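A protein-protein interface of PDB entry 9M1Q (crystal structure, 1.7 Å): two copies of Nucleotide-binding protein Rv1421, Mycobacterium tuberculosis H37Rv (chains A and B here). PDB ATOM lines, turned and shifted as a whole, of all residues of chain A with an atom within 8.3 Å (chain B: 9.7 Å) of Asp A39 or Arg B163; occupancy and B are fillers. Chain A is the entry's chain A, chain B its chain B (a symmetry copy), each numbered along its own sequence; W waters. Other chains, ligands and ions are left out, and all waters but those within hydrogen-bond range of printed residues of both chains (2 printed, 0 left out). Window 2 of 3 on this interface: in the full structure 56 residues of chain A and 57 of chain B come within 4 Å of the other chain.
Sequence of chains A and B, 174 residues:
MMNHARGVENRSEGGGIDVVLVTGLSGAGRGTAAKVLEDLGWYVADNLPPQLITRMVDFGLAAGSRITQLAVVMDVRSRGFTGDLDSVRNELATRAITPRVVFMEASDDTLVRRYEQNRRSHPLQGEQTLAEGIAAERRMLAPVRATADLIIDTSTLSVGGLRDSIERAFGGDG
The backbone carbonyl oxygen (O) of Leu A37 lies within hydrogen-bond range of the backbone NH (N) of Trp A42 (3.0 Å). OG of Ser B165 sits at hydrogen-bond distance from O of Leu B162. The guanidinium group (NE) of Arg B163 lies within salt-bridge range of the side-chain carboxylate (OE2) of Glu B167.
No position is printed for both chains. Of the 16 pairs that touch across the chains among the printed residues, none has its exchanged pair printed and touching as well.
Printed residues of chain B within 4 Å of Thr A32: Leu B162 (3.3 Å), Arg B163 (3.8 Å) and Ile B166 (3.6 Å). Of chain B, only Arg B163, Ile B166 and Phe B170 come within 4 Å of Val A36. Of the printed residues of chain B, Leu A37 touches Phe B170. Asp A39 touches just one residue of chain B: Arg B163. No residue of chain B comes within 4 Å of Leu A40. Of the printed residues of chain B, Met A104 touches Ile B152, Thr B154 and Ile B166. Printed residues of chain A within 4 Å of Leu B162: Thr A32 (3.3 Å). Arg B163 touches three residues of chain A. Printed residues of chain A within 4 Å of Ile B166: Gly A29, Thr A32, Ala A33, Val A36 and Met A104. The nearest residue of chain B that does not touch Asp A39 is Glu B167 (5.7 Å). The nearest residue of chain A that does not touch Arg B163 is Lys A35 (4.3 Å).
Of the 17 printed residues of chain B, 7 touch a printed residue of chain A. Hydrophobic or aromatic side chains of chain B that line the printed part of chain A: Ile B152, Leu B157, Leu B162, Ile B166 and Phe B170. Of the 17 printed residues of chain A, 8 touch a printed residue of chain B.
OD2 of Asp A39 is in salt-bridge range of NH2 of Arg B163 (2.8 Å). NH2 of Arg A114 lies within hydrogen-bond range of O of Thr B154 (2.8 Å). The guanidinium group (NH2) of Arg A114 is in hydrogen-bond range of the backbone carbonyl oxygen (O) of Leu B157 (3.0 Å).
Gly A29 touches Ile B166 (O to CD1, 3.8 Å). Thr A32 touches Leu B162 (OG1 to CD2, 3.3 Å). CG2 of Thr A32 touches CA of Arg B163 (3.8 Å). Thr A32 touches Ile B166 (CG2 to CD1, 3.6 Å). Ala A33 touches Ile B166 (N to CD1, 3.7 Å). O of Ala A33 touches CE2 of Phe B170, at 3.8 Å. Val A36 touches Arg B163. Val A36 touches Ile B166 (CG2 to CG2, 3.9 Å). Phe B170 touches Val A36. CE2 of Phe B170 touches CG of Leu A37, 3.6 Å away.
Water W2 lies within hydrogen-bond range of the backbone carbonyl oxygen (O) of Leu B157 (2.7 Å) and the guanidinium group (NE) of Arg A114 (2.8 Å). Water W1 bridges the backbone carbonyl oxygen (O) of Val B159 (2.7 Å) and the side-chain hydroxyl (OG1) of Thr A32 (3.0 Å).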
ATOM      1  N   GLY A  29     -24.970 -12.843 -28.033  1.00  0.00           N
ATOM      2  CA  GLY A  29     -24.379 -13.047 -26.723  1.00  0.00           C
ATOM      3  C   GLY A  29     -23.955 -11.822 -25.944  1.00  0.00           C
ATOM      4  O   GLY A  29     -23.135 -11.941 -25.030  1.00  0.00           O
ATOM      5  N   GLY A  31     -25.692 -10.176 -23.757  1.00  0.00           N
ATOM      6  CA  GLY A  31     -26.108 -10.375 -22.374  1.00  0.00           C
ATOM      7  C   GLY A  31     -25.163 -11.259 -21.574  1.00  0.00           C
ATOM      8  O   GLY A  31     -24.834 -10.957 -20.421  1.00  0.00           O
ATOM      9  N   THR A  32     -24.721 -12.369 -22.167  1.00  0.00           N
ATOM     10  CA  THR A  32     -23.751 -13.224 -21.491  1.00  0.00           C
ATOM     11  C   THR A  32     -22.414 -12.513 -21.322  1.00  0.00           C
ATOM     12  O   THR A  32     -21.777 -12.643 -20.281  1.00  0.00           O
ATOM     13  CB  THR A  32     -23.583 -14.550 -22.254  1.00  0.00           C
ATOM     14  OG1 THR A  32     -24.820 -15.265 -22.244  1.00  0.00           O
ATOM     15  CG2 THR A  32     -22.538 -15.458 -21.614  1.00  0.00           C
ATOM     16  N   ALA A  33     -21.982 -11.728 -22.318  1.00  0.00           N
ATOM     17  CA  ALA A  33     -20.734 -10.986 -22.140  1.00  0.00           C
ATOM     18  C   ALA A  33     -20.829 -10.018 -20.959  1.00  0.00           C
ATOM     19  O   ALA A  33     -19.869  -9.859 -20.198  1.00  0.00           O
ATOM     20  CB  ALA A  33     -20.370 -10.234 -23.425  1.00  0.00           C
ATOM     21  N   ALA A  34     -21.978  -9.365 -20.793  1.00  0.00           N
ATOM     22  CA  ALA A  34     -22.139  -8.432 -19.682  1.00  0.00           C
ATOM     23  C   ALA A  34     -22.116  -9.173 -18.352  1.00  0.00           C
ATOM     24  O   ALA A  34     -21.499  -8.707 -17.387  1.00  0.00           O
ATOM     25  CB  ALA A  34     -23.437  -7.635 -19.851  1.00  0.00           C
ATOM     26  N   LYS A  35     -22.724 -10.354 -18.306  1.00  0.00           N
ATOM     27  CA  LYS A  35     -22.712 -11.160 -17.087  1.00  0.00           C
ATOM     28  C   LYS A  35     -21.303 -11.621 -16.738  1.00  0.00           C
ATOM     29  O   LYS A  35     -20.910 -11.591 -15.561  1.00  0.00           O
ATOM     30  CB  LYS A  35     -23.636 -12.369 -17.241  1.00  0.00           C
ATOM     31  CG  LYS A  35     -25.118 -12.096 -17.040  1.00  0.00           C
ATOM     32  CD  LYS A  35     -25.872 -13.417 -17.050  1.00  0.00           C
ATOM     33  CE  LYS A  35     -27.287 -13.267 -16.540  1.00  0.00           C
ATOM     34  NZ  LYS A  35     -28.134 -12.479 -17.479  1.00  0.00           N
ATOM     35  N   VAL A  36     -20.526 -12.065 -17.741  1.00  0.00           N
ATOM     36  CA  VAL A  36     -19.143 -12.457 -17.481  1.00  0.00           C
ATOM     37  C   VAL A  36     -18.345 -11.276 -16.942  1.00  0.00           C
ATOM     38  O   VAL A  36     -17.579 -11.420 -15.984  1.00  0.00           O
ATOM     39  CB  VAL A  36     -18.474 -13.062 -18.737  1.00  0.00           C
ATOM     40  CG1 VAL A  36     -16.985 -13.281 -18.468  1.00  0.00           C
ATOM     41  CG2 VAL A  36     -19.138 -14.404 -19.120  1.00  0.00           C
ATOM     42  N   LEU A  37     -18.513 -10.094 -17.539  1.00  0.00           N
ATOM     43  CA  LEU A  37     -17.772  -8.923 -17.066  1.00  0.00           C
ATOM     44  C   LEU A  37     -18.190  -8.539 -15.648  1.00  0.00           C
ATOM     45  O   LEU A  37     -17.349  -8.174 -14.822  1.00  0.00           O
ATOM     46  CB  LEU A  37     -17.982  -7.745 -18.017  1.00  0.00           C
ATOM     47  CG  LEU A  37     -17.252  -7.893 -19.352  1.00  0.00           C
ATOM     48  CD1 LEU A  37     -17.789  -6.880 -20.364  1.00  0.00           C
ATOM     49  CD2 LEU A  37     -15.758  -7.680 -19.122  1.00  0.00           C
ATOM     50  N   GLU A  38     -19.488  -8.577 -15.358  1.00  0.00           N
ATOM     51  CA  GLU A  38     -19.928  -8.294 -13.993  1.00  0.00           C
ATOM     52  C   GLU A  38     -19.285  -9.264 -13.008  1.00  0.00           C
ATOM     53  O   GLU A  38     -18.792  -8.857 -11.943  1.00  0.00           O
ATOM     54  CB  GLU A  38     -21.455  -8.360 -13.931  1.00  0.00           C
ATOM     55  CG  GLU A  38     -22.074  -7.829 -12.654  1.00  0.00           C
ATOM     56  CD  GLU A  38     -23.565  -7.588 -12.805  1.00  0.00           C
ATOM     57  OE1 GLU A  38     -23.945  -6.599 -13.467  1.00  0.00           O
ATOM     58  OE2 GLU A  38     -24.353  -8.388 -12.268  1.00  0.00           O
ATOM     59  N   ASP A  39     -19.240 -10.550 -13.376  1.00  0.00           N
ATOM     60  CA  ASP A  39     -18.630 -11.574 -12.530  1.00  0.00           C
ATOM     61  C   ASP A  39     -17.142 -11.328 -12.309  1.00  0.00           C
ATOM     62  O   ASP A  39     -16.602 -11.697 -11.255  1.00  0.00           O
ATOM     63  CB  ASP A  39     -18.838 -12.959 -13.154  1.00  0.00           C
ATOM     64  CG  ASP A  39     -20.273 -13.444 -13.062  1.00  0.00           C
ATOM     65  OD1 ASP A  39     -21.113 -12.772 -12.422  1.00  0.00           O
ATOM     66  OD2 ASP A  39     -20.577 -14.516 -13.630  1.00  0.00           O
ATOM     67  N   LEU A  40     -16.452 -10.745 -13.297  1.00  0.00           N
ATOM     68  CA  LEU A  40     -15.037 -10.417 -13.179  1.00  0.00           C
ATOM     69  C   LEU A  40     -14.800  -9.121 -12.423  1.00  0.00           C
ATOM     70  O   LEU A  40     -13.643  -8.723 -12.270  1.00  0.00           O
ATOM     71  CB  LEU A  40     -14.394 -10.320 -14.573  1.00  0.00           C
ATOM     72  CG  LEU A  40     -14.280 -11.622 -15.372  1.00  0.00           C
ATOM     73  CD1 LEU A  40     -13.899 -11.356 -16.815  1.00  0.00           C
ATOM     74  CD2 LEU A  40     -13.292 -12.623 -14.725  1.00  0.00           C
ATOM     75  N   GLY A  41     -15.860  -8.438 -11.979  1.00  0.00           N
ATOM     76  CA  GLY A  41     -15.735  -7.264 -11.137  1.00  0.00           C
ATOM     77  C   GLY A  41     -16.032  -5.948 -11.815  1.00  0.00           C
ATOM     78  O   GLY A  41     -15.920  -4.900 -11.171  1.00  0.00           O
ATOM     79  N   TRP A  42     -16.417  -5.961 -13.086  1.00  0.00           N
ATOM     80  CA  TRP A  42     -16.767  -4.736 -13.784  1.00  0.00           C
ATOM     81  C   TRP A  42     -18.112  -4.213 -13.307  1.00  0.00           C
ATOM     82  O   TRP A  42     -19.025  -4.978 -12.997  1.00  0.00           O
ATOM     83  CB  TRP A  42     -16.817  -5.001 -15.299  1.00  0.00           C
ATOM     84  CG  TRP A  42     -15.479  -5.306 -15.808  1.00  0.00           C
ATOM     85  CD1 TRP A  42     -14.766  -6.453 -15.616  1.00  0.00           C
ATOM     86  CD2 TRP A  42     -14.653  -4.440 -16.570  1.00  0.00           C
ATOM     87  NE1 TRP A  42     -13.541  -6.354 -16.219  1.00  0.00           N
ATOM     88  CE2 TRP A  42     -13.440  -5.117 -16.801  1.00  0.00           C
ATOM     89  CE3 TRP A  42     -14.819  -3.156 -17.086  1.00  0.00           C
ATOM     90  CZ2 TRP A  42     -12.407  -4.560 -17.538  1.00  0.00           C
ATOM     91  CZ3 TRP A  42     -13.775  -2.596 -17.810  1.00  0.00           C
ATOM     92  CH2 TRP A  42     -12.583  -3.295 -18.016  1.00  0.00           C
ATOM     93  N   TYR A  43     -18.237  -2.893 -13.253  1.00  0.00           N
ATOM     94  CA  TYR A  43     -19.544  -2.269 -13.116  1.00  0.00           C
ATOM     95  C   TYR A  43     -20.139  -2.145 -14.514  1.00  0.00           C
ATOM     96  O   TYR A  43     -19.534  -1.529 -15.396  1.00  0.00           O
ATOM     97  CB  TYR A  43     -19.442  -0.907 -12.435  1.00  0.00           C
ATOM     98  CG  TYR A  43     -20.777  -0.224 -12.242  1.00  0.00           C
ATOM     99  CD1 TYR A  43     -21.288   0.625 -13.209  1.00  0.00           C
ATOM    100  CD2 TYR A  43     -21.526  -0.427 -11.086  1.00  0.00           C
ATOM    101  CE1 TYR A  43     -22.509   1.254 -13.043  1.00  0.00           C
ATOM    102  CE2 TYR A  43     -22.755   0.200 -10.911  1.00  0.00           C
ATOM    103  CZ  TYR A  43     -23.232   1.041 -11.889  1.00  0.00           C
ATOM    104  OH  TYR A  43     -24.447   1.668 -11.730  1.00  0.00           O
ATOM    105  N   VAL A  44     -21.311  -2.737 -14.726  1.00  0.00           N
ATOM    106  CA  VAL A  44     -21.896  -2.841 -16.058  1.00  0.00           C
ATOM    107  C   VAL A  44     -23.096  -1.912 -16.155  1.00  0.00           C
ATOM    108  O   VAL A  44     -24.094  -2.085 -15.438  1.00  0.00           O
ATOM    109  CB  VAL A  44     -22.288  -4.290 -16.389  1.00  0.00           C
ATOM    110  CG1 VAL A  44     -22.928  -4.363 -17.773  1.00  0.00           C
ATOM    111  CG2 VAL A  44     -21.073  -5.186 -16.305  1.00  0.00           C
ATOM    112  N   MET A 104     -20.066  -8.894 -30.630  1.00  0.00           N
ATOM    113  CA  MET A 104     -20.621 -10.252 -30.605  1.00  0.00           C
ATOM    114  C   MET A 104     -21.347 -10.526 -31.916  1.00  0.00           C
ATOM    115  O   MET A 104     -22.221  -9.754 -32.313  1.00  0.00           O
ATOM    116  CB  MET A 104     -21.592 -10.433 -29.423  1.00  0.00           C
ATOM    117  CG  MET A 104     -21.071  -9.960 -28.050  1.00  0.00           C
ATOM    118  SD  MET A 104     -19.605 -10.919 -27.534  1.00  0.00           S
ATOM    119  CE  MET A 104     -20.268 -12.554 -27.405  1.00  0.00           C
ATOM    120  N   ARG A 114     -31.555 -19.152 -31.880  1.00  0.00           N
ATOM    121  CA  ARG A 114     -31.669 -18.522 -30.568  1.00  0.00           C
ATOM    122  C   ARG A 114     -32.944 -17.700 -30.437  1.00  0.00           C
ATOM    123  O   ARG A 114     -33.558 -17.667 -29.360  1.00  0.00           O
ATOM    124  CB  ARG A 114     -30.450 -17.658 -30.292  1.00  0.00           C
ATOM    125  CG  ARG A 114     -29.203 -18.521 -30.130  1.00  0.00           C
ATOM    126  CD  ARG A 114     -28.090 -17.781 -29.442  1.00  0.00           C
ATOM    127  NE  ARG A 114     -26.916 -18.639 -29.331  1.00  0.00           N
ATOM    128  CZ  ARG A 114     -25.702 -18.287 -29.747  1.00  0.00           C
ATOM    129  NH1 ARG A 114     -25.443 -17.063 -30.193  1.00  0.00           N
ATOM    130  NH2 ARG A 114     -24.719 -19.182 -29.702  1.00  0.00           N
ATOM    131  N   ILE B 152     -16.214 -11.809 -31.098  1.00  0.00           N
ATOM    132  CA  ILE B 152     -16.507 -13.148 -30.593  1.00  0.00           C
ATOM    133  C   ILE B 152     -17.623 -13.713 -31.444  1.00  0.00           C
ATOM    134  O   ILE B 152     -18.740 -13.180 -31.435  1.00  0.00           O
ATOM    135  CB  ILE B 152     -16.905 -13.149 -29.103  1.00  0.00           C
ATOM    136  CG1 ILE B 152     -15.819 -12.479 -28.249  1.00  0.00           C
ATOM    137  CG2 ILE B 152     -17.125 -14.597 -28.659  1.00  0.00           C
ATOM    138  CD1 ILE B 152     -16.155 -12.352 -26.740  1.00  0.00           C
ATOM    139  N   THR B 154     -20.149 -16.578 -31.976  1.00  0.00           N
ATOM    140  CA  THR B 154     -20.772 -17.592 -31.146  1.00  0.00           C
ATOM    141  C   THR B 154     -21.608 -18.577 -31.954  1.00  0.00           C
ATOM    142  O   THR B 154     -22.483 -19.256 -31.389  1.00  0.00           O
ATOM    143  CB  THR B 154     -21.595 -16.921 -30.038  1.00  0.00           C
ATOM    144  OG1 THR B 154     -22.675 -16.189 -30.628  1.00  0.00           O
ATOM    145  CG2 THR B 154     -20.695 -15.931 -29.284  1.00  0.00           C
ATOM    146  N   LEU B 157     -23.057 -22.398 -30.833  1.00  0.00           N
ATOM    147  CA  LEU B 157     -22.812 -22.666 -29.422  1.00  0.00           C
ATOM    148  C   LEU B 157     -24.115 -22.785 -28.642  1.00  0.00           C
ATOM    149  O   LEU B 157     -25.065 -22.018 -28.846  1.00  0.00           O
ATOM    150  CB  LEU B 157     -21.939 -21.574 -28.811  1.00  0.00           C
ATOM    151  CG  LEU B 157     -20.530 -21.430 -29.376  1.00  0.00           C
ATOM    152  CD1 LEU B 157     -19.805 -20.339 -28.646  1.00  0.00           C
ATOM    153  CD2 LEU B 157     -19.787 -22.766 -29.243  1.00  0.00           C
ATOM    154  N   SER B 158     -24.141 -23.740 -27.713  1.00  0.00           N
ATOM    155  CA  SER B 158     -25.228 -23.836 -26.755  1.00  0.00           C
ATOM    156  C   SER B 158     -25.157 -22.673 -25.769  1.00  0.00           C
ATOM    157  O   SER B 158     -24.207 -21.887 -25.770  1.00  0.00           O
ATOM    158  CB  SER B 158     -25.131 -25.156 -25.992  1.00  0.00           C
ATOM    159  OG  SER B 158     -23.898 -25.160 -25.288  1.00  0.00           O
ATOM    160  N   VAL B 159     -26.174 -22.570 -24.905  1.00  0.00           N
ATOM    161  CA  VAL B 159     -26.159 -21.547 -23.859  1.00  0.00           C
ATOM    162  C   VAL B 159     -24.887 -21.660 -23.029  1.00  0.00           C
ATOM    163  O   VAL B 159     -24.202 -20.663 -22.752  1.00  0.00           O
ATOM    164  CB  VAL B 159     -27.421 -21.653 -22.979  1.00  0.00           C
ATOM    165  CG1 VAL B 159     -27.309 -20.736 -21.780  1.00  0.00           C
ATOM    166  CG2 VAL B 159     -28.679 -21.324 -23.795  1.00  0.00           C
ATOM    167  N   GLY B 160     -24.532 -22.883 -22.641  1.00  0.00           N
ATOM    168  CA  GLY B 160     -23.325 -23.063 -21.856  1.00  0.00           C
ATOM    169  C   GLY B 160     -22.059 -22.835 -22.665  1.00  0.00           C
ATOM    170  O   GLY B 160     -21.073 -22.300 -22.148  1.00  0.00           O
ATOM    171  N   GLY B 161     -22.058 -23.268 -23.929  1.00  0.00           N
ATOM    172  CA  GLY B 161     -20.881 -23.085 -24.765  1.00  0.00           C
ATOM    173  C   GLY B 161     -20.630 -21.629 -25.070  1.00  0.00           C
ATOM    174  O   GLY B 161     -19.476 -21.194 -25.155  1.00  0.00           O
ATOM    175  N   LEU B 162     -21.703 -20.854 -25.198  1.00  0.00           N
ATOM    176  CA  LEU B 162     -21.598 -19.403 -25.296  1.00  0.00           C
ATOM    177  C   LEU B 162     -20.854 -18.825 -24.094  1.00  0.00           C
ATOM    178  O   LEU B 162     -19.912 -18.035 -24.244  1.00  0.00           O
ATOM    179  CB  LEU B 162     -23.015 -18.819 -25.403  1.00  0.00           C
ATOM    180  CG  LEU B 162     -23.196 -17.305 -25.344  1.00  0.00           C
ATOM    181  CD1 LEU B 162     -22.747 -16.762 -26.657  1.00  0.00           C
ATOM    182  CD2 LEU B 162     -24.666 -16.933 -25.119  1.00  0.00           C
ATOM    183  N   ARG B 163     -21.251 -19.233 -22.880  1.00  0.00           N
ATOM    184  CA  ARG B 163     -20.609 -18.743 -21.671  1.00  0.00           C
ATOM    185  C   ARG B 163     -19.126 -19.125 -21.638  1.00  0.00           C
ATOM    186  O   ARG B 163     -18.268 -18.285 -21.334  1.00  0.00           O
ATOM    187  CB  ARG B 163     -21.352 -19.297 -20.451  1.00  0.00           C
ATOM    188  CG  ARG B 163     -20.644 -19.088 -19.129  1.00  0.00           C
ATOM    189  CD  ARG B 163     -20.891 -17.719 -18.547  1.00  0.00           C
ATOM    190  NE  ARG B 163     -20.063 -17.494 -17.363  1.00  0.00           N
ATOM    191  CZ  ARG B 163     -20.370 -16.661 -16.377  1.00  0.00           C
ATOM    192  NH1 ARG B 163     -21.542 -16.054 -16.326  1.00  0.00           N
ATOM    193  NH2 ARG B 163     -19.467 -16.414 -15.429  1.00  0.00           N
ATOM    194  N   ASP B 164     -18.810 -20.386 -21.969  1.00  0.00           N
ATOM    195  CA  ASP B 164     -17.414 -20.840 -21.964  1.00  0.00           C
ATOM    196  C   ASP B 164     -16.565 -20.036 -22.944  1.00  0.00           C
ATOM    197  O   ASP B 164     -15.422 -19.664 -22.634  1.00  0.00           O
ATOM    198  CB  ASP B 164     -17.334 -22.321 -22.340  1.00  0.00           C
ATOM    199  CG  ASP B 164     -17.639 -23.268 -21.174  1.00  0.00           C
ATOM    200  OD1 ASP B 164     -17.585 -22.852 -19.998  1.00  0.00           O
ATOM    201  OD2 ASP B 164     -17.914 -24.457 -21.466  1.00  0.00           O
ATOM    202  N   SER B 165     -17.097 -19.780 -24.142  1.00  0.00           N
ATOM    203  CA  SER B 165     -16.312 -19.091 -25.165  1.00  0.00           C
ATOM    204  C   SER B 165     -16.018 -17.657 -24.755  1.00  0.00           C
ATOM    205  O   SER B 165     -14.916 -17.140 -24.993  1.00  0.00           O
ATOM    206  CB  SER B 165     -17.040 -19.149 -26.518  1.00  0.00           C
ATOM    207  OG  SER B 165     -18.184 -18.286 -26.545  1.00  0.00           O
ATOM    208  N   ILE B 166     -16.975 -17.003 -24.101  1.00  0.00           N
ATOM    209  CA  ILE B 166     -16.746 -15.640 -23.661  1.00  0.00           C
ATOM    210  C   ILE B 166     -15.770 -15.601 -22.485  1.00  0.00           C
ATOM    211  O   ILE B 166     -14.889 -14.738 -22.430  1.00  0.00           O
ATOM    212  CB  ILE B 166     -18.093 -14.969 -23.336  1.00  0.00           C
ATOM    213  CG1 ILE B 166     -18.951 -14.879 -24.610  1.00  0.00           C
ATOM    214  CG2 ILE B 166     -17.857 -13.600 -22.726  1.00  0.00           C
ATOM    215  CD1 ILE B 166     -20.406 -14.466 -24.307  1.00  0.00           C
ATOM    216  N   GLU B 167     -15.918 -16.516 -21.519  1.00  0.00           N
ATOM    217  CA  GLU B 167     -14.948 -16.600 -20.432  1.00  0.00           C
ATOM    218  C   GLU B 167     -13.542 -16.789 -20.964  1.00  0.00           C
ATOM    219  O   GLU B 167     -12.596 -16.149 -20.479  1.00  0.00           O
ATOM    220  CB  GLU B 167     -15.318 -17.740 -19.477  1.00  0.00           C
ATOM    221  CG  GLU B 167     -16.538 -17.437 -18.667  1.00  0.00           C
ATOM    222  CD  GLU B 167     -16.833 -18.513 -17.600  1.00  0.00           C
ATOM    223  OE1 GLU B 167     -16.159 -19.561 -17.591  1.00  0.00           O
ATOM    224  OE2 GLU B 167     -17.732 -18.290 -16.776  1.00  0.00           O
ATOM    225  N   ARG B 168     -13.380 -17.646 -21.972  1.00  0.00           N
ATOM    226  CA  ARG B 168     -12.053 -17.871 -22.536  1.00  0.00           C
ATOM    227  C   ARG B 168     -11.545 -16.622 -23.243  1.00  0.00           C
ATOM    228  O   ARG B 168     -10.373 -16.247 -23.098  1.00  0.00           O
ATOM    229  CB  ARG B 168     -12.082 -19.043 -23.518  1.00  0.00           C
ATOM    230  CG  ARG B 168     -12.423 -20.406 -22.933  1.00  0.00           C
ATOM    231  CD  ARG B 168     -12.315 -21.496 -24.007  1.00  0.00           C
ATOM    232  NE  ARG B 168     -13.564 -22.231 -24.195  1.00  0.00           N
ATOM    233  CZ  ARG B 168     -14.291 -22.221 -25.305  1.00  0.00           C
ATOM    234  NH1 ARG B 168     -13.902 -21.554 -26.385  1.00  0.00           N
ATOM    235  NH2 ARG B 168     -15.429 -22.910 -25.339  1.00  0.00           N
ATOM    236  N   ALA B 169     -12.417 -15.974 -24.026  1.00  0.00           N
ATOM    237  CA  ALA B 169     -12.033 -14.765 -24.746  1.00  0.00           C
ATOM    238  C   ALA B 169     -11.634 -13.635 -23.805  1.00  0.00           C
ATOM    239  O   ALA B 169     -10.762 -12.824 -24.152  1.00  0.00           O
ATOM    240  CB  ALA B 169     -13.181 -14.326 -25.660  1.00  0.00           C
ATOM    241  N   PHE B 170     -12.248 -13.549 -22.625  1.00  0.00           N
ATOM    242  CA  PHE B 170     -11.959 -12.465 -21.698  1.00  0.00           C
ATOM    243  C   PHE B 170     -10.832 -12.801 -20.736  1.00  0.00           C
ATOM    244  O   PHE B 170     -10.519 -11.977 -19.871  1.00  0.00           O
ATOM    245  CB  PHE B 170     -13.190 -12.071 -20.872  1.00  0.00           C
ATOM    246  CG  PHE B 170     -14.247 -11.329 -21.640  1.00  0.00           C
ATOM    247  CD1 PHE B 170     -14.022 -10.896 -22.940  1.00  0.00           C
ATOM    248  CD2 PHE B 170     -15.477 -11.066 -21.059  1.00  0.00           C
ATOM    249  CE1 PHE B 170     -15.015 -10.232 -23.644  1.00  0.00           C
ATOM    250  CE2 PHE B 170     -16.469 -10.397 -21.748  1.00  0.00           C
ATOM    251  CZ  PHE B 170     -16.244  -9.970 -23.038  1.00  0.00           C
ATOM    252  N   GLY B 171     -10.236 -13.984 -20.849  1.00  0.00           N
ATOM    253  CA  GLY B 171      -9.112 -14.364 -20.006  1.00  0.00           C
ATOM    254  C   GLY B 171      -9.445 -15.485 -19.040  1.00  0.00           C
ATOM    255  O   GLY B 171      -9.506 -16.656 -19.429  1.00  0.00           O
HETATM  256  O   HOH W   1     -24.962 -18.204 -21.868  1.00  0.00           O
HETATM  257  O   HOH W   2     -27.338 -20.964 -27.862  1.00  0.00           O
